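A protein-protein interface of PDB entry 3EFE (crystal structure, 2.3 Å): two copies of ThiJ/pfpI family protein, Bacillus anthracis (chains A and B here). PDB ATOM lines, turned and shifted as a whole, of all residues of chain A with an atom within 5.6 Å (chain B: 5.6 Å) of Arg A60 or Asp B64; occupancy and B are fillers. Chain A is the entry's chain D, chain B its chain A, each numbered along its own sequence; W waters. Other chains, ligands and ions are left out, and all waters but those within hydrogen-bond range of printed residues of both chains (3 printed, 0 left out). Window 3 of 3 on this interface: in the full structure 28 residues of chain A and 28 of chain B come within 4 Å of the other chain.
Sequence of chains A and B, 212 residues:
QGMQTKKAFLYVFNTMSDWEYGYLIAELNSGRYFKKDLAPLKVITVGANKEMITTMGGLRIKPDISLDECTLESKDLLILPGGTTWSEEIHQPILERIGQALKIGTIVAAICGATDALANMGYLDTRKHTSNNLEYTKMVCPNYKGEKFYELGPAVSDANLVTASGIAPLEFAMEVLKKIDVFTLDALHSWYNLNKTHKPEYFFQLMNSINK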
ATOM      1  N   MET A  52       8.893   0.593  -8.349  1.00  0.00           N
ATOM      2  CA  MET A  52      10.005  -0.082  -7.724  1.00  0.00           C
ATOM      3  C   MET A  52      10.333   0.556  -6.410  1.00  0.00           C
ATOM      4  O   MET A  52      10.256   1.814  -6.241  1.00  0.00           O
ATOM      5  CB  MET A  52      11.216  -0.061  -8.676  1.00  0.00           C
ATOM      6  CG  MET A  52      10.946  -1.010  -9.884  1.00  0.00           C
ATOM      7  SD  MET A  52      12.367  -1.826 -10.537  1.00  0.00           S
ATOM      8  CE  MET A  52      12.674  -2.846  -9.125  1.00  0.00           C
ATOM      9  N   ILE A  53      10.675  -0.321  -5.472  1.00  0.00           N
ATOM     10  CA  ILE A  53      11.017  -0.004  -4.088  1.00  0.00           C
ATOM     11  C   ILE A  53      12.438  -0.472  -3.905  1.00  0.00           C
ATOM     12  O   ILE A  53      12.954  -1.245  -4.693  1.00  0.00           O
ATOM     13  CB  ILE A  53      10.015  -0.655  -3.107  1.00  0.00           C
ATOM     14  CG1 ILE A  53      10.181  -2.183  -2.955  1.00  0.00           C
ATOM     15  CG2 ILE A  53       8.610  -0.418  -3.621  1.00  0.00           C
ATOM     16  CD1 ILE A  53      11.254  -2.661  -2.033  1.00  0.00           C
ATOM     17  N   THR A  54      13.099   0.066  -2.905  1.00  0.00           N
ATOM     18  CA  THR A  54      14.483  -0.243  -2.555  1.00  0.00           C
ATOM     19  C   THR A  54      14.471  -0.706  -1.053  1.00  0.00           C
ATOM     20  O   THR A  54      13.963   0.005  -0.161  1.00  0.00           O
ATOM     21  CB  THR A  54      15.345   1.014  -2.704  1.00  0.00           C
ATOM     22  OG1 THR A  54      15.252   1.506  -4.047  1.00  0.00           O
ATOM     23  CG2 THR A  54      16.840   0.707  -2.390  1.00  0.00           C
ATOM     24  N   THR A  55      14.959  -1.897  -0.773  1.00  0.00           N
ATOM     25  CA  THR A  55      14.950  -2.371   0.622  1.00  0.00           C
ATOM     26  C   THR A  55      15.927  -1.561   1.431  1.00  0.00           C
ATOM     27  O   THR A  55      16.685  -0.855   0.859  1.00  0.00           O
ATOM     28  CB  THR A  55      15.221  -3.913   0.743  1.00  0.00           C
ATOM     29  OG1 THR A  55      16.551  -4.197   0.358  1.00  0.00           O
ATOM     30  CG2 THR A  55      14.236  -4.727  -0.134  1.00  0.00           C
ATOM     31  N   GLY A  58      19.120  -2.265   0.166  1.00  0.00           N
ATOM     32  CA  GLY A  58      19.471  -1.646  -1.114  1.00  0.00           C
ATOM     33  C   GLY A  58      19.007  -2.423  -2.303  1.00  0.00           C
ATOM     34  O   GLY A  58      19.423  -2.150  -3.401  1.00  0.00           O
ATOM     35  N   LEU A  59      18.139  -3.423  -2.110  1.00  0.00           N
ATOM     36  CA  LEU A  59      17.699  -4.239  -3.222  1.00  0.00           C
ATOM     37  C   LEU A  59      16.549  -3.557  -3.935  1.00  0.00           C
ATOM     38  O   LEU A  59      15.595  -3.233  -3.310  1.00  0.00           O
ATOM     39  CB  LEU A  59      17.279  -5.591  -2.711  1.00  0.00           C
ATOM     40  CG  LEU A  59      18.246  -6.464  -1.904  1.00  0.00           C
ATOM     41  CD1 LEU A  59      17.387  -7.696  -1.493  1.00  0.00           C
ATOM     42  CD2 LEU A  59      19.530  -6.831  -2.719  1.00  0.00           C
ATOM     43  N   ARG A  60      16.640  -3.332  -5.246  1.00  0.00           N
ATOM     44  CA  ARG A  60      15.531  -2.714  -6.003  1.00  0.00           C
ATOM     45  C   ARG A  60      14.546  -3.765  -6.501  1.00  0.00           C
ATOM     46  O   ARG A  60      14.876  -4.588  -7.319  1.00  0.00           O
ATOM     47  CB  ARG A  60      16.024  -1.884  -7.176  1.00  0.00           C
ATOM     48  CG  ARG A  60      17.277  -1.017  -6.902  1.00  0.00           C
ATOM     49  CD  ARG A  60      17.053   0.505  -6.724  1.00  0.00           C
ATOM     50  NE  ARG A  60      15.788   1.010  -7.305  1.00  0.00           N
ATOM     51  CZ  ARG A  60      15.371   0.902  -8.579  1.00  0.00           C
ATOM     52  NH1 ARG A  60      14.182   1.431  -8.902  1.00  0.00           N
ATOM     53  NH2 ARG A  60      16.081   0.258  -9.520  1.00  0.00           N
ATOM     54  N   ILE A  61      13.323  -3.710  -6.005  1.00  0.00           N
ATOM     55  CA  ILE A  61      12.357  -4.741  -6.255  1.00  0.00           C
ATOM     56  C   ILE A  61      11.144  -4.208  -7.013  1.00  0.00           C
ATOM     57  O   ILE A  61      10.628  -3.153  -6.705  1.00  0.00           O
ATOM     58  CB  ILE A  61      11.914  -5.383  -4.874  1.00  0.00           C
ATOM     59  CG1 ILE A  61      13.131  -6.084  -4.242  1.00  0.00           C
ATOM     60  CG2 ILE A  61      10.658  -6.285  -5.024  1.00  0.00           C
ATOM     61  CD1 ILE A  61      12.929  -6.481  -2.739  1.00  0.00           C
ATOM     62  N   LYS A  62      10.638  -5.000  -7.927  1.00  0.00           N
ATOM     63  CA  LYS A  62       9.501  -4.646  -8.749  1.00  0.00           C
ATOM     64  C   LYS A  62       8.312  -5.315  -8.144  1.00  0.00           C
ATOM     65  O   LYS A  62       8.260  -6.559  -8.128  1.00  0.00           O
ATOM     66  CB  LYS A  62       9.730  -5.152 -10.193  1.00  0.00           C
ATOM     67  CG  LYS A  62       8.659  -4.783 -11.251  1.00  0.00           C
ATOM     68  CD  LYS A  62       8.341  -3.233 -11.267  1.00  0.00           C
ATOM     69  CE  LYS A  62       7.284  -2.797 -12.372  1.00  0.00           C
ATOM     70  NZ  LYS A  62       7.248  -3.754 -13.535  1.00  0.00           N
ATOM     71  N   VAL B  43      25.413  -1.164  -0.820  1.00  0.00           N
ATOM     72  CA  VAL B  43      25.422  -2.496  -1.385  1.00  0.00           C
ATOM     73  C   VAL B  43      24.975  -2.477  -2.857  1.00  0.00           C
ATOM     74  O   VAL B  43      23.810  -2.324  -3.178  1.00  0.00           O
ATOM     75  CB  VAL B  43      24.583  -3.428  -0.476  1.00  0.00           C
ATOM     76  CG1 VAL B  43      24.478  -4.836  -1.124  1.00  0.00           C
ATOM     77  CG2 VAL B  43      25.246  -3.461   0.881  1.00  0.00           C
ATOM     78  N   ILE B  44      25.939  -2.550  -3.762  1.00  0.00           N
ATOM     79  CA  ILE B  44      25.634  -2.565  -5.213  1.00  0.00           C
ATOM     80  C   ILE B  44      25.345  -4.028  -5.606  1.00  0.00           C
ATOM     81  O   ILE B  44      26.138  -4.900  -5.286  1.00  0.00           O
ATOM     82  CB  ILE B  44      26.801  -1.936  -6.070  1.00  0.00           C
ATOM     83  CG1 ILE B  44      27.065  -0.476  -5.600  1.00  0.00           C
ATOM     84  CG2 ILE B  44      26.502  -2.020  -7.603  1.00  0.00           C
ATOM     85  CD1 ILE B  44      28.521   0.051  -5.953  1.00  0.00           C
ATOM     86  N   THR B  45      24.163  -4.259  -6.174  1.00  0.00           N
ATOM     87  CA  THR B  45      23.782  -5.548  -6.676  1.00  0.00           C
ATOM     88  C   THR B  45      24.381  -5.757  -8.073  1.00  0.00           C
ATOM     89  O   THR B  45      24.270  -4.900  -8.940  1.00  0.00           O
ATOM     90  CB  THR B  45      22.246  -5.781  -6.741  1.00  0.00           C
ATOM     91  OG1 THR B  45      21.652  -4.870  -7.665  1.00  0.00           O
ATOM     92  CG2 THR B  45      21.546  -5.719  -5.314  1.00  0.00           C
ATOM     93  N   VAL B  46      25.032  -6.906  -8.236  1.00  0.00           N
ATOM     94  CA  VAL B  46      25.752  -7.317  -9.399  1.00  0.00           C
ATOM     95  C   VAL B  46      25.186  -8.662  -9.907  1.00  0.00           C
ATOM     96  O   VAL B  46      25.323  -9.686  -9.271  1.00  0.00           O
ATOM     97  CB  VAL B  46      27.283  -7.492  -9.072  1.00  0.00           C
ATOM     98  CG1 VAL B  46      27.845  -6.408  -8.257  1.00  0.00           C
ATOM     99  CG2 VAL B  46      27.515  -8.749  -8.364  1.00  0.00           C
ATOM    100  N   GLY B  47      24.511  -8.647 -11.041  1.00  0.00           N
ATOM    101  CA  GLY B  47      24.057  -9.852 -11.684  1.00  0.00           C
ATOM    102  C   GLY B  47      25.047 -10.370 -12.738  1.00  0.00           C
ATOM    103  O   GLY B  47      25.972  -9.654 -13.136  1.00  0.00           O
ATOM    104  N   ARG B  60      11.422 -10.119  -7.073  1.00  0.00           N
ATOM    105  CA  ARG B  60      12.009  -9.759  -8.372  1.00  0.00           C
ATOM    106  C   ARG B  60      12.960  -8.569  -8.300  1.00  0.00           C
ATOM    107  O   ARG B  60      12.548  -7.432  -8.189  1.00  0.00           O
ATOM    108  CB  ARG B  60      10.907  -9.521  -9.401  1.00  0.00           C
ATOM    109  CG  ARG B  60       9.920 -10.649  -9.487  1.00  0.00           C
ATOM    110  CD  ARG B  60       9.708 -11.011 -10.935  1.00  0.00           C
ATOM    111  NE  ARG B  60      10.937 -11.567 -11.511  1.00  0.00           N
ATOM    112  CZ  ARG B  60      11.308 -11.476 -12.786  1.00  0.00           C
ATOM    113  NH1 ARG B  60      12.441 -12.041 -13.164  1.00  0.00           N
ATOM    114  NH2 ARG B  60      10.583 -10.808 -13.671  1.00  0.00           N
ATOM    115  N   ILE B  61      14.244  -8.859  -8.410  1.00  0.00           N
ATOM    116  CA  ILE B  61      15.257  -7.879  -8.158  1.00  0.00           C
ATOM    117  C   ILE B  61      15.924  -7.460  -9.495  1.00  0.00           C
ATOM    118  O   ILE B  61      16.158  -8.263 -10.364  1.00  0.00           O
ATOM    119  CB  ILE B  61      16.322  -8.371  -7.110  1.00  0.00           C
ATOM    120  CG1 ILE B  61      15.676  -8.641  -5.738  1.00  0.00           C
ATOM    121  CG2 ILE B  61      17.478  -7.340  -6.995  1.00  0.00           C
ATOM    122  CD1 ILE B  61      16.536  -9.473  -4.824  1.00  0.00           C
ATOM    123  N   LYS B  62      16.207  -6.167  -9.614  1.00  0.00           N
ATOM    124  CA  LYS B  62      16.751  -5.596 -10.803  1.00  0.00           C
ATOM    125  C   LYS B  62      18.198  -5.318 -10.492  1.00  0.00           C
ATOM    126  O   LYS B  62      18.492  -4.401  -9.675  1.00  0.00           O
ATOM    127  CB  LYS B  62      15.994  -4.303 -11.103  1.00  0.00           C
ATOM    128  CG  LYS B  62      16.653  -3.413 -12.143  1.00  0.00           C
ATOM    129  CD  LYS B  62      16.668  -4.051 -13.531  1.00  0.00           C
ATOM    130  CE  LYS B  62      17.081  -3.009 -14.609  1.00  0.00           C
ATOM    131  NZ  LYS B  62      16.125  -1.824 -14.603  1.00  0.00           N
ATOM    132  N   PRO B  63      19.116  -6.099 -11.098  1.00  0.00           N
ATOM    133  CA  PRO B  63      20.527  -5.900 -10.793  1.00  0.00           C
ATOM    134  C   PRO B  63      20.996  -4.454 -11.016  1.00  0.00           C
ATOM    135  O   PRO B  63      20.608  -3.835 -12.028  1.00  0.00           O
ATOM    136  CB  PRO B  63      21.219  -6.817 -11.786  1.00  0.00           C
ATOM    137  CG  PRO B  63      20.251  -7.938 -12.003  1.00  0.00           C
ATOM    138  CD  PRO B  63      18.922  -7.217 -12.036  1.00  0.00           C
ATOM    139  N   ASP B  64      21.828  -3.911 -10.117  1.00  0.00           N
ATOM    140  CA  ASP B  64      22.370  -2.589 -10.387  1.00  0.00           C
ATOM    141  C   ASP B  64      23.276  -2.613 -11.598  1.00  0.00           C
ATOM    142  O   ASP B  64      23.147  -1.808 -12.497  1.00  0.00           O
ATOM    143  CB  ASP B  64      23.073  -2.014  -9.196  1.00  0.00           C
ATOM    144  CG  ASP B  64      22.077  -1.706  -8.003  1.00  0.00           C
ATOM    145  OD1 ASP B  64      20.823  -1.617  -8.232  1.00  0.00           O
ATOM    146  OD2 ASP B  64      22.589  -1.569  -6.871  1.00  0.00           O
ATOM    147  N   ILE B  65      24.200  -3.553 -11.602  1.00  0.00           N
ATOM    148  CA  ILE B  65      25.180  -3.658 -12.625  1.00  0.00           C
ATOM    149  C   ILE B  65      25.307  -5.133 -13.069  1.00  0.00           C
ATOM    150  O   ILE B  65      24.847  -6.052 -12.362  1.00  0.00           O
ATOM    151  CB  ILE B  65      26.505  -2.967 -12.197  1.00  0.00           C
ATOM    152  CG1 ILE B  65      27.259  -3.746 -11.134  1.00  0.00           C
ATOM    153  CG2 ILE B  65      26.182  -1.527 -11.658  1.00  0.00           C
ATOM    154  CD1 ILE B  65      28.527  -3.051 -10.685  1.00  0.00           C
ATOM    155  N   SER B  66      25.850  -5.321 -14.286  1.00  0.00           N
ATOM    156  CA  SER B  66      26.245  -6.640 -14.791  1.00  0.00           C
ATOM    157  C   SER B  66      27.654  -6.875 -14.279  1.00  0.00           C
ATOM    158  O   SER B  66      28.344  -5.909 -13.871  1.00  0.00           O
ATOM    159  CB  SER B  66      26.195  -6.702 -16.317  1.00  0.00           C
ATOM    160  OG  SER B  66      27.079  -5.772 -16.911  1.00  0.00           O
ATOM    161  N   GLU B  69      30.426  -4.867 -15.880  1.00  0.00           N
ATOM    162  CA  GLU B  69      30.528  -3.469 -15.452  1.00  0.00           C
ATOM    163  C   GLU B  69      31.211  -3.374 -14.112  1.00  0.00           C
ATOM    164  O   GLU B  69      31.486  -2.247 -13.637  1.00  0.00           O
ATOM    165  CB  GLU B  69      29.157  -2.791 -15.339  1.00  0.00           C
ATOM    166  CG  GLU B  69      28.420  -2.628 -16.668  1.00  0.00           C
ATOM    167  CD  GLU B  69      26.933  -2.216 -16.520  1.00  0.00           C
ATOM    168  OE1 GLU B  69      26.305  -2.387 -15.445  1.00  0.00           O
ATOM    169  OE2 GLU B  69      26.370  -1.703 -17.511  1.00  0.00           O
HETATM  170  O   HOH W   1      18.588  -1.740  -9.991  1.00  0.00           O
HETATM  171  O   HOH W   2      19.275  -4.034  -6.926  1.00  0.00           O
HETATM  172  O   HOH W   3       8.812  -8.680  -6.558  1.00  0.00           O
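N of Leu A59 sits at hydrogen-bond distance from OG1 of Thr A55 (3.0 Å). O of Ile A53 sits at hydrogen-bond distance from N of Ile A61 (2.8 Å). O of Thr B45 sits at hydrogen-bond distance from N of Ile B65 (3.0 Å). OG1 of Thr A54 lies within hydrogen-bond range of NE of Arg A60 (3.3 Å). N of Asp B64 is in hydrogen-bond range of OG1 of Thr B45 (2.6 Å).
Water W2 lies within hydrogen-bond range of OG1 of Thr B45 (2.6 Å), O of Lys B62 (2.9 Å), OD1 of Asp B64 (3.2 Å) and N of Arg A60 (3.2 Å). Water W1 lies within hydrogen-bond range of O of Lys B62 (2.7 Å), OD1 of Asp B64 (2.8 Å) and NH2 of Arg A60 (3.2 Å). Water W3 bridges the backbone carbonyl oxygen (O) of Lys A62 (2.7 Å) and the backbone NH (N) of Arg B60 (3.0 Å).
Arg A60 touches its own counterpart, Arg B60. Arg A60 touches Ile B61, and with the chains exchanged Ile A61 touches Arg B60. Arg A60 touches Lys B62, and with the chains exchanged Lys A62 touches Arg B60. Ile B61 touches its own counterpart, Ile A61. Positions printed for both chains: 60, 61 and 62.
The backbone NH (N) of Lys B62 is in hydrogen-bond range of the backbone carbonyl oxygen (O) of Arg A60 (3.1 Å). O of Arg B60 sits at hydrogen-bond distance from N of Lys A62, 3.1 Å away.
Of the 9 printed residues of chain A, 4 touch a printed residue of chain B. Printed residues of chain B that touch a printed residue of chain A: Thr B45, Arg B60, Ile B61, Lys B62 and Asp B64. Hydrophobic or aromatic side chains of chain B within 4 Å of the printed part of chain A: Ile B61. Along chain B the printed residues that touch a printed residue of chain A span positions 45 to 64.
Ile A53 touches none of the printed residues of chain B. Gly A58 touches none of the printed residues of chain B. Of the printed residues of chain B, Leu A59 touches Thr B45 and Ile B61. Of the printed residues of chain B, Arg A60 touches Arg B60 (3.8 Å), Ile B61 (3.4 Å), Lys B62 (3.1 Å) and Asp B64 (3.8 Å). Printed residues of chain A within 4 Å of Thr B45: Leu A59 (3.5 Å). Of the printed residues of chain A, Arg B60 touches Arg A60, Ile A61 and Lys A62. Printed residues of chain A within 4 Å of Ile B61: Leu A59 (3.9 Å), Arg A60 (3.4 Å) and Ile A61 (3.9 Å). Of the printed residues of chain A, Lys B62 touches Arg A60. Asp B64 touches just one residue of chain A: Arg A60 (3.8 Å). The nearest printed residue of chain A that does not touch Thr B45 is Gly A58 (4.6 Å).
Leu A59 touches Thr B45. Ile B61 touches Leu A59 (CD1 to CD1, 3.9 Å). Arg B60 touches Arg A60. Arg A60 touches Ile B61. Asp B64 touches Arg A60 (OD1 to CG, 3.8 Å). Ile A61 touches Arg B60 (CA to O, 3.3 Å). Ile A61 touches Ile B61.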
